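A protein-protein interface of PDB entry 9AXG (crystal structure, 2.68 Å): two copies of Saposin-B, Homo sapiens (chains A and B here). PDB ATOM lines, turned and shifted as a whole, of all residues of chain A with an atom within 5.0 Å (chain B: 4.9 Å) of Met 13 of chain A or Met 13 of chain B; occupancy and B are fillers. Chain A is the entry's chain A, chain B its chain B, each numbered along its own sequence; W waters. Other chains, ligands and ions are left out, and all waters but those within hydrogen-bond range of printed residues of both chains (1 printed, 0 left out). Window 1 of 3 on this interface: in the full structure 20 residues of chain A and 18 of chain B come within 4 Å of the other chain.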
ATOM      1  N   VAL A   6      15.403 -22.611  24.815  1.00  0.00           N
ATOM      2  CA  VAL A   6      15.169 -23.761  23.947  1.00  0.00           C
ATOM      3  C   VAL A   6      14.046 -24.631  24.500  1.00  0.00           C
ATOM      4  O   VAL A   6      13.204 -25.136  23.745  1.00  0.00           O
ATOM      5  CB  VAL A   6      16.487 -24.541  23.781  1.00  0.00           C
ATOM      6  CG1 VAL A   6      16.264 -25.976  23.341  1.00  0.00           C
ATOM      7  CG2 VAL A   6      17.395 -23.819  22.809  1.00  0.00           C
ATOM      8  N   ASP A   9      10.758 -22.851  23.816  1.00  0.00           N
ATOM      9  CA  ASP A   9      10.497 -22.943  22.385  1.00  0.00           C
ATOM     10  C   ASP A   9       9.999 -24.325  22.003  1.00  0.00           C
ATOM     11  O   ASP A   9       9.101 -24.462  21.165  1.00  0.00           O
ATOM     12  CB  ASP A   9      11.767 -22.619  21.607  1.00  0.00           C
ATOM     13  CG  ASP A   9      12.174 -21.176  21.733  1.00  0.00           C
ATOM     14  OD1 ASP A   9      11.339 -20.334  22.119  1.00  0.00           O
ATOM     15  OD2 ASP A   9      13.359 -20.895  21.495  1.00  0.00           O
ATOM     16  N   CYS A  10      10.580 -25.362  22.613  1.00  0.00           N
ATOM     17  CA  CYS A  10      10.152 -26.730  22.354  1.00  0.00           C
ATOM     18  C   CYS A  10       8.732 -26.976  22.832  1.00  0.00           C
ATOM     19  O   CYS A  10       7.971 -27.673  22.152  1.00  0.00           O
ATOM     20  CB  CYS A  10      11.099 -27.718  23.023  1.00  0.00           C
ATOM     21  SG  CYS A  10      10.630 -29.449  22.744  1.00  0.00           S
ATOM     22  N   ILE A  11       8.378 -26.476  24.023  1.00  0.00           N
ATOM     23  CA  ILE A  11       7.004 -26.649  24.507  1.00  0.00           C
ATOM     24  C   ILE A  11       6.023 -25.935  23.587  1.00  0.00           C
ATOM     25  O   ILE A  11       4.953 -26.474  23.262  1.00  0.00           O
ATOM     26  CB  ILE A  11       6.857 -26.174  25.964  1.00  0.00           C
ATOM     27  CG1 ILE A  11       7.841 -26.902  26.880  1.00  0.00           C
ATOM     28  CG2 ILE A  11       5.430 -26.380  26.465  1.00  0.00           C
ATOM     29  CD1 ILE A  11       7.881 -26.342  28.297  1.00  0.00           C
ATOM     30  N   GLN A  12       6.396 -24.735  23.125  1.00  0.00           N
ATOM     31  CA  GLN A  12       5.604 -23.999  22.142  1.00  0.00           C
ATOM     32  C   GLN A  12       5.421 -24.816  20.860  1.00  0.00           C
ATOM     33  O   GLN A  12       4.295 -24.956  20.346  1.00  0.00           O
ATOM     34  CB  GLN A  12       6.303 -22.662  21.864  1.00  0.00           C
ATOM     35  CG  GLN A  12       5.530 -21.602  21.107  1.00  0.00           C
ATOM     36  CD  GLN A  12       4.030 -21.683  21.305  1.00  0.00           C
ATOM     37  OE1 GLN A  12       3.311 -22.143  20.427  1.00  0.00           O
ATOM     38  NE2 GLN A  12       3.546 -21.191  22.442  1.00  0.00           N
ATOM     39  N   MET A  13       6.512 -25.434  20.385  1.00  0.00           N
ATOM     40  CA  MET A  13       6.463 -26.236  19.167  1.00  0.00           C
ATOM     41  C   MET A  13       5.607 -27.479  19.325  1.00  0.00           C
ATOM     42  O   MET A  13       4.817 -27.801  18.436  1.00  0.00           O
ATOM     43  CB  MET A  13       7.855 -26.659  18.716  1.00  0.00           C
ATOM     44  CG  MET A  13       7.855 -26.937  17.227  1.00  0.00           C
ATOM     45  SD  MET A  13       9.423 -27.454  16.591  1.00  0.00           S
ATOM     46  CE  MET A  13       9.737 -28.876  17.637  1.00  0.00           C
ATOM     47  N   VAL A  14       5.786 -28.218  20.418  1.00  0.00           N
ATOM     48  CA  VAL A  14       5.052 -29.469  20.579  1.00  0.00           C
ATOM     49  C   VAL A  14       3.569 -29.191  20.814  1.00  0.00           C
ATOM     50  O   VAL A  14       2.705 -29.926  20.304  1.00  0.00           O
ATOM     51  CB  VAL A  14       5.700 -30.320  21.693  1.00  0.00           C
ATOM     52  CG1 VAL A  14       4.929 -31.587  21.927  1.00  0.00           C
ATOM     53  CG2 VAL A  14       7.130 -30.692  21.289  1.00  0.00           C
ATOM     54  N   THR A  15       3.248 -28.096  21.524  1.00  0.00           N
ATOM     55  CA  THR A  15       1.859 -27.677  21.699  1.00  0.00           C
ATOM     56  C   THR A  15       1.198 -27.366  20.361  1.00  0.00           C
ATOM     57  O   THR A  15       0.091 -27.844  20.074  1.00  0.00           O
ATOM     58  CB  THR A  15       1.804 -26.453  22.613  1.00  0.00           C
ATOM     59  OG1 THR A  15       2.334 -26.786  23.902  1.00  0.00           O
ATOM     60  CG2 THR A  15       0.380 -25.946  22.761  1.00  0.00           C
ATOM     61  N   ASP A  16       1.889 -26.614  19.500  1.00  0.00           N
ATOM     62  CA  ASP A  16       1.300 -26.330  18.198  1.00  0.00           C
ATOM     63  C   ASP A  16       1.323 -27.529  17.256  1.00  0.00           C
ATOM     64  O   ASP A  16       0.490 -27.592  16.347  1.00  0.00           O
ATOM     65  CB  ASP A  16       1.994 -25.143  17.548  1.00  0.00           C
ATOM     66  CG  ASP A  16       1.651 -23.848  18.227  1.00  0.00           C
ATOM     67  OD1 ASP A  16       0.727 -23.853  19.069  1.00  0.00           O
ATOM     68  OD2 ASP A  16       2.258 -22.817  17.889  1.00  0.00           O
ATOM     69  N   ILE A  17       2.225 -28.490  17.460  1.00  0.00           N
ATOM     70  CA  ILE A  17       2.196 -29.709  16.658  1.00  0.00           C
ATOM     71  C   ILE A  17       0.981 -30.556  17.019  1.00  0.00           C
ATOM     72  O   ILE A  17       0.276 -31.058  16.134  1.00  0.00           O
ATOM     73  CB  ILE A  17       3.515 -30.485  16.821  1.00  0.00           C
ATOM     74  CG1 ILE A  17       4.595 -29.874  15.933  1.00  0.00           C
ATOM     75  CG2 ILE A  17       3.352 -31.938  16.436  1.00  0.00           C
ATOM     76  CD1 ILE A  17       6.002 -30.215  16.371  1.00  0.00           C
ATOM     77  N   PHE A  79      15.383 -31.237  25.319  1.00  0.00           N
ATOM     78  CA  PHE A  79      15.447 -29.784  25.317  1.00  0.00           C
ATOM     79  C   PHE A  79      14.941 -29.162  26.610  1.00  0.00           C
ATOM     80  O   PHE A  79      15.155 -27.962  26.817  1.00  0.00           O
ATOM     81  CB  PHE A  79      14.662 -29.244  24.124  1.00  0.00           C
ATOM     82  CG  PHE A  79      15.244 -29.634  22.796  1.00  0.00           C
ATOM     83  CD1 PHE A  79      16.595 -29.487  22.547  1.00  0.00           C
ATOM     84  CD2 PHE A  79      14.445 -30.164  21.806  1.00  0.00           C
ATOM     85  CE1 PHE A  79      17.133 -29.844  21.329  1.00  0.00           C
ATOM     86  CE2 PHE A  79      14.977 -30.523  20.581  1.00  0.00           C
ATOM     87  CZ  PHE A  79      16.321 -30.368  20.345  1.00  0.00           C
ATOM     88  N   VAL B   6       3.581 -24.072  13.533  1.00  0.00           N
ATOM     89  CA  VAL B   6       4.615 -25.083  13.744  1.00  0.00           C
ATOM     90  C   VAL B   6       5.915 -24.676  13.048  1.00  0.00           C
ATOM     91  O   VAL B   6       7.007 -24.801  13.618  1.00  0.00           O
ATOM     92  CB  VAL B   6       4.105 -26.457  13.261  1.00  0.00           C
ATOM     93  CG1 VAL B   6       5.234 -27.482  13.193  1.00  0.00           C
ATOM     94  CG2 VAL B   6       2.972 -26.950  14.149  1.00  0.00           C
ATOM     95  N   ASP B   9       7.480 -21.845  15.078  1.00  0.00           N
ATOM     96  CA  ASP B   9       8.063 -22.416  16.289  1.00  0.00           C
ATOM     97  C   ASP B   9       9.373 -23.134  15.993  1.00  0.00           C
ATOM     98  O   ASP B   9      10.320 -23.064  16.788  1.00  0.00           O
ATOM     99  CB  ASP B   9       7.091 -23.401  16.935  1.00  0.00           C
ATOM    100  CG  ASP B   9       5.844 -22.760  17.479  1.00  0.00           C
ATOM    101  OD1 ASP B   9       4.951 -23.522  17.894  1.00  0.00           O
ATOM    102  OD2 ASP B   9       5.752 -21.525  17.513  1.00  0.00           O
ATOM    103  N   CYS B  10       9.435 -23.828  14.850  1.00  0.00           N
ATOM    104  CA  CYS B  10      10.654 -24.524  14.457  1.00  0.00           C
ATOM    105  C   CYS B  10      11.788 -23.552  14.178  1.00  0.00           C
ATOM    106  O   CYS B  10      12.922 -23.808  14.596  1.00  0.00           O
ATOM    107  CB  CYS B  10      10.413 -25.404  13.230  1.00  0.00           C
ATOM    108  SG  CYS B  10      11.872 -26.398  12.762  1.00  0.00           S
ATOM    109  N   ILE B  11      11.511 -22.460  13.443  1.00  0.00           N
ATOM    110  CA  ILE B  11      12.566 -21.483  13.134  1.00  0.00           C
ATOM    111  C   ILE B  11      13.117 -20.878  14.416  1.00  0.00           C
ATOM    112  O   ILE B  11      14.338 -20.817  14.621  1.00  0.00           O
ATOM    113  CB  ILE B  11      12.056 -20.364  12.209  1.00  0.00           C
ATOM    114  CG1 ILE B  11      11.374 -20.901  10.938  1.00  0.00           C
ATOM    115  CG2 ILE B  11      13.208 -19.398  11.892  1.00  0.00           C
ATOM    116  CD1 ILE B  11      12.255 -21.184   9.771  1.00  0.00           C
ATOM    117  N   GLN B  12      12.213 -20.469  15.312  1.00  0.00           N
ATOM    118  CA  GLN B  12      12.619 -19.896  16.589  1.00  0.00           C
ATOM    119  C   GLN B  12      13.418 -20.887  17.432  1.00  0.00           C
ATOM    120  O   GLN B  12      14.460 -20.532  18.004  1.00  0.00           O
ATOM    121  CB  GLN B  12      11.384 -19.420  17.343  1.00  0.00           C
ATOM    122  CG  GLN B  12      11.700 -18.628  18.588  1.00  0.00           C
ATOM    123  CD  GLN B  12      10.446 -18.155  19.273  1.00  0.00           C
ATOM    124  OE1 GLN B  12       9.560 -17.585  18.633  1.00  0.00           O
ATOM    125  NE2 GLN B  12      10.350 -18.397  20.578  1.00  0.00           N
ATOM    126  N   MET B  13      12.985 -22.148  17.470  1.00  0.00           N
ATOM    127  CA  MET B  13      13.664 -23.123  18.312  1.00  0.00           C
ATOM    128  C   MET B  13      15.019 -23.505  17.742  1.00  0.00           C
ATOM    129  O   MET B  13      15.988 -23.654  18.487  1.00  0.00           O
ATOM    130  CB  MET B  13      12.793 -24.358  18.486  1.00  0.00           C
ATOM    131  CG  MET B  13      13.436 -25.449  19.294  1.00  0.00           C
ATOM    132  SD  MET B  13      12.337 -26.829  19.406  1.00  0.00           S
ATOM    133  CE  MET B  13      13.262 -28.020  18.437  1.00  0.00           C
ATOM    134  N   VAL B  14      15.114 -23.661  16.428  1.00  0.00           N
ATOM    135  CA  VAL B  14      16.375 -24.079  15.840  1.00  0.00           C
ATOM    136  C   VAL B  14      17.376 -22.932  15.896  1.00  0.00           C
ATOM    137  O   VAL B  14      18.573 -23.149  16.135  1.00  0.00           O
ATOM    138  CB  VAL B  14      16.128 -24.609  14.410  1.00  0.00           C
ATOM    139  CG1 VAL B  14      17.413 -24.698  13.583  1.00  0.00           C
ATOM    140  CG2 VAL B  14      15.418 -25.961  14.478  1.00  0.00           C
ATOM    141  N   THR B  15      16.895 -21.688  15.751  1.00  0.00           N
ATOM    142  CA  THR B  15      17.773 -20.536  15.937  1.00  0.00           C
ATOM    143  C   THR B  15      18.281 -20.450  17.375  1.00  0.00           C
ATOM    144  O   THR B  15      19.477 -20.205  17.609  1.00  0.00           O
ATOM    145  CB  THR B  15      17.046 -19.254  15.547  1.00  0.00           C
ATOM    146  OG1 THR B  15      16.424 -19.427  14.268  1.00  0.00           O
ATOM    147  CG2 THR B  15      18.025 -18.100  15.473  1.00  0.00           C
ATOM    148  N   ASP B  16      17.405 -20.706  18.353  1.00  0.00           N
ATOM    149  CA  ASP B  16      17.876 -20.688  19.730  1.00  0.00           C
ATOM    150  C   ASP B  16      18.740 -21.898  20.072  1.00  0.00           C
ATOM    151  O   ASP B  16      19.611 -21.785  20.940  1.00  0.00           O
ATOM    152  CB  ASP B  16      16.697 -20.554  20.684  1.00  0.00           C
ATOM    153  CG  ASP B  16      16.220 -19.127  20.782  1.00  0.00           C
ATOM    154  OD1 ASP B  16      15.036 -18.856  20.524  1.00  0.00           O
ATOM    155  OD2 ASP B  16      17.063 -18.249  21.068  1.00  0.00           O
ATOM    156  N   ILE B  17      18.573 -23.018  19.367  1.00  0.00           N
ATOM    157  CA  ILE B  17      19.459 -24.171  19.537  1.00  0.00           C
ATOM    158  C   ILE B  17      20.853 -23.865  18.996  1.00  0.00           C
ATOM    159  O   ILE B  17      21.872 -24.212  19.621  1.00  0.00           O
ATOM    160  CB  ILE B  17      18.829 -25.409  18.867  1.00  0.00           C
ATOM    161  CG1 ILE B  17      17.826 -26.071  19.816  1.00  0.00           C
ATOM    162  CG2 ILE B  17      19.875 -26.438  18.428  1.00  0.00           C
ATOM    163  CD1 ILE B  17      16.857 -26.969  19.099  1.00  0.00           C
ATOM    164  N   PHE B  79       8.775 -29.451   9.071  1.00  0.00           N
ATOM    165  CA  PHE B  79       7.913 -28.477   9.728  1.00  0.00           C
ATOM    166  C   PHE B  79       7.736 -27.207   8.914  1.00  0.00           C
ATOM    167  O   PHE B  79       6.825 -26.428   9.212  1.00  0.00           O
ATOM    168  CB  PHE B  79       8.459 -28.125  11.110  1.00  0.00           C
ATOM    169  CG  PHE B  79       8.446 -29.273  12.071  1.00  0.00           C
ATOM    170  CD1 PHE B  79       7.444 -30.229  12.018  1.00  0.00           C
ATOM    171  CD2 PHE B  79       9.452 -29.416  13.008  1.00  0.00           C
ATOM    172  CE1 PHE B  79       7.435 -31.300  12.900  1.00  0.00           C
ATOM    173  CE2 PHE B  79       9.459 -30.487  13.888  1.00  0.00           C
ATOM    174  CZ  PHE B  79       8.448 -31.430  13.835  1.00  0.00           C
HETATM  175  O   HOH W   1       9.071 -22.576  19.443  1.00  0.00           O
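The side-chain amide oxygen (OE1) of Gln 12 of chain A sits close to the side-chain carboxylate (OD2) of Asp 16 of chain A.
Of chain B, only Asp 9, Cys 10 and Met 13 come within 4 Å of Met 13 of chain A. Met 13 of chain B touches four residues of chain A. Printed residues of chain B within 4 Å of Val 6 of chain A: Asp 16 and Ile 17. Of the printed residues of chain A, Asp 9 of chain B touches Gln 12, Met 13 and Asp 16. Thr 15 of chain A touches none of the printed residues of chain B. The nearest residue of chain B that does not touch Met 13 of chain A is Phe 79 of chain B (4.1 Å).
Water W1 lies within hydrogen-bond range of O of Asp 9 of chain A (2.6 Å) and O of Asp 9 of chain B (3.0 Å).
The side-chain carboxylate (OD2) of Asp 9 of chain A lies close to the side-chain carboxylate (OD1) of Asp 16 of chain B (2.8 Å). The side-chain carboxylate (OD1) of Asp 9 of chain B sits close to the side-chain carboxylate (OD2) of Asp 16 of chain A (2.8 Å). The side-chain amide nitrogen (NE2) of Gln 12 of chain B lies within hydrogen-bond range of the side-chain carboxylate (OD1) of Asp 9 of chain A (2.7 Å). The side-chain amide oxygen of Gln 12 of chain A lies close to the side-chain carboxylate of Asp 9 of chain B (3.3 Å).
Among the printed residues, merely in contact across the chains: Met 13 of chain A with Asp 9 of chain B, Asp 16 of chain A with Val 6 of chain B, Val 6 of chain A with Asp 16 of chain B, Phe 79 of chain A with Ile 17 of chain B, Cys 10 of chain A with Met 13 of chain B, Ile 17 of chain A with Val 6 of chain B, Met 13 of chain A with Met 13 of chain B, Phe 79 of chain A with Met 13 of chain B, Asp 9 of chain A with Met 13 of chain B, Val 6 of chain A with Ile 17 of chain B, Ile 17 of chain A with Phe 79 of chain B and Met 13 of chain A with Cys 10 of chain B.
Of the 11 printed residues of chain B, 8 touch a printed residue of chain A. Printed residues of chain A that touch a printed residue of chain B: Val 6, Asp 9, Cys 10, Gln 12, Met 13, Asp 16, Ile 17 and Phe 79.
Val 6 of chain A touches Ile 17 of chain B, and with the chains exchanged Ile 17 of chain A touches Val 6 of chain B. Asp 9 of chain A touches Gln 12 of chain B, and with the chains exchanged Gln 12 of chain A touches Asp 9 of chain B. Met 13 of chain A touches its own counterpart, Met 13 of chain B. Ile 17 of chain A touches Phe 79 of chain B, and with the chains exchanged Phe 79 of chain A touches Ile 17 of chain B.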
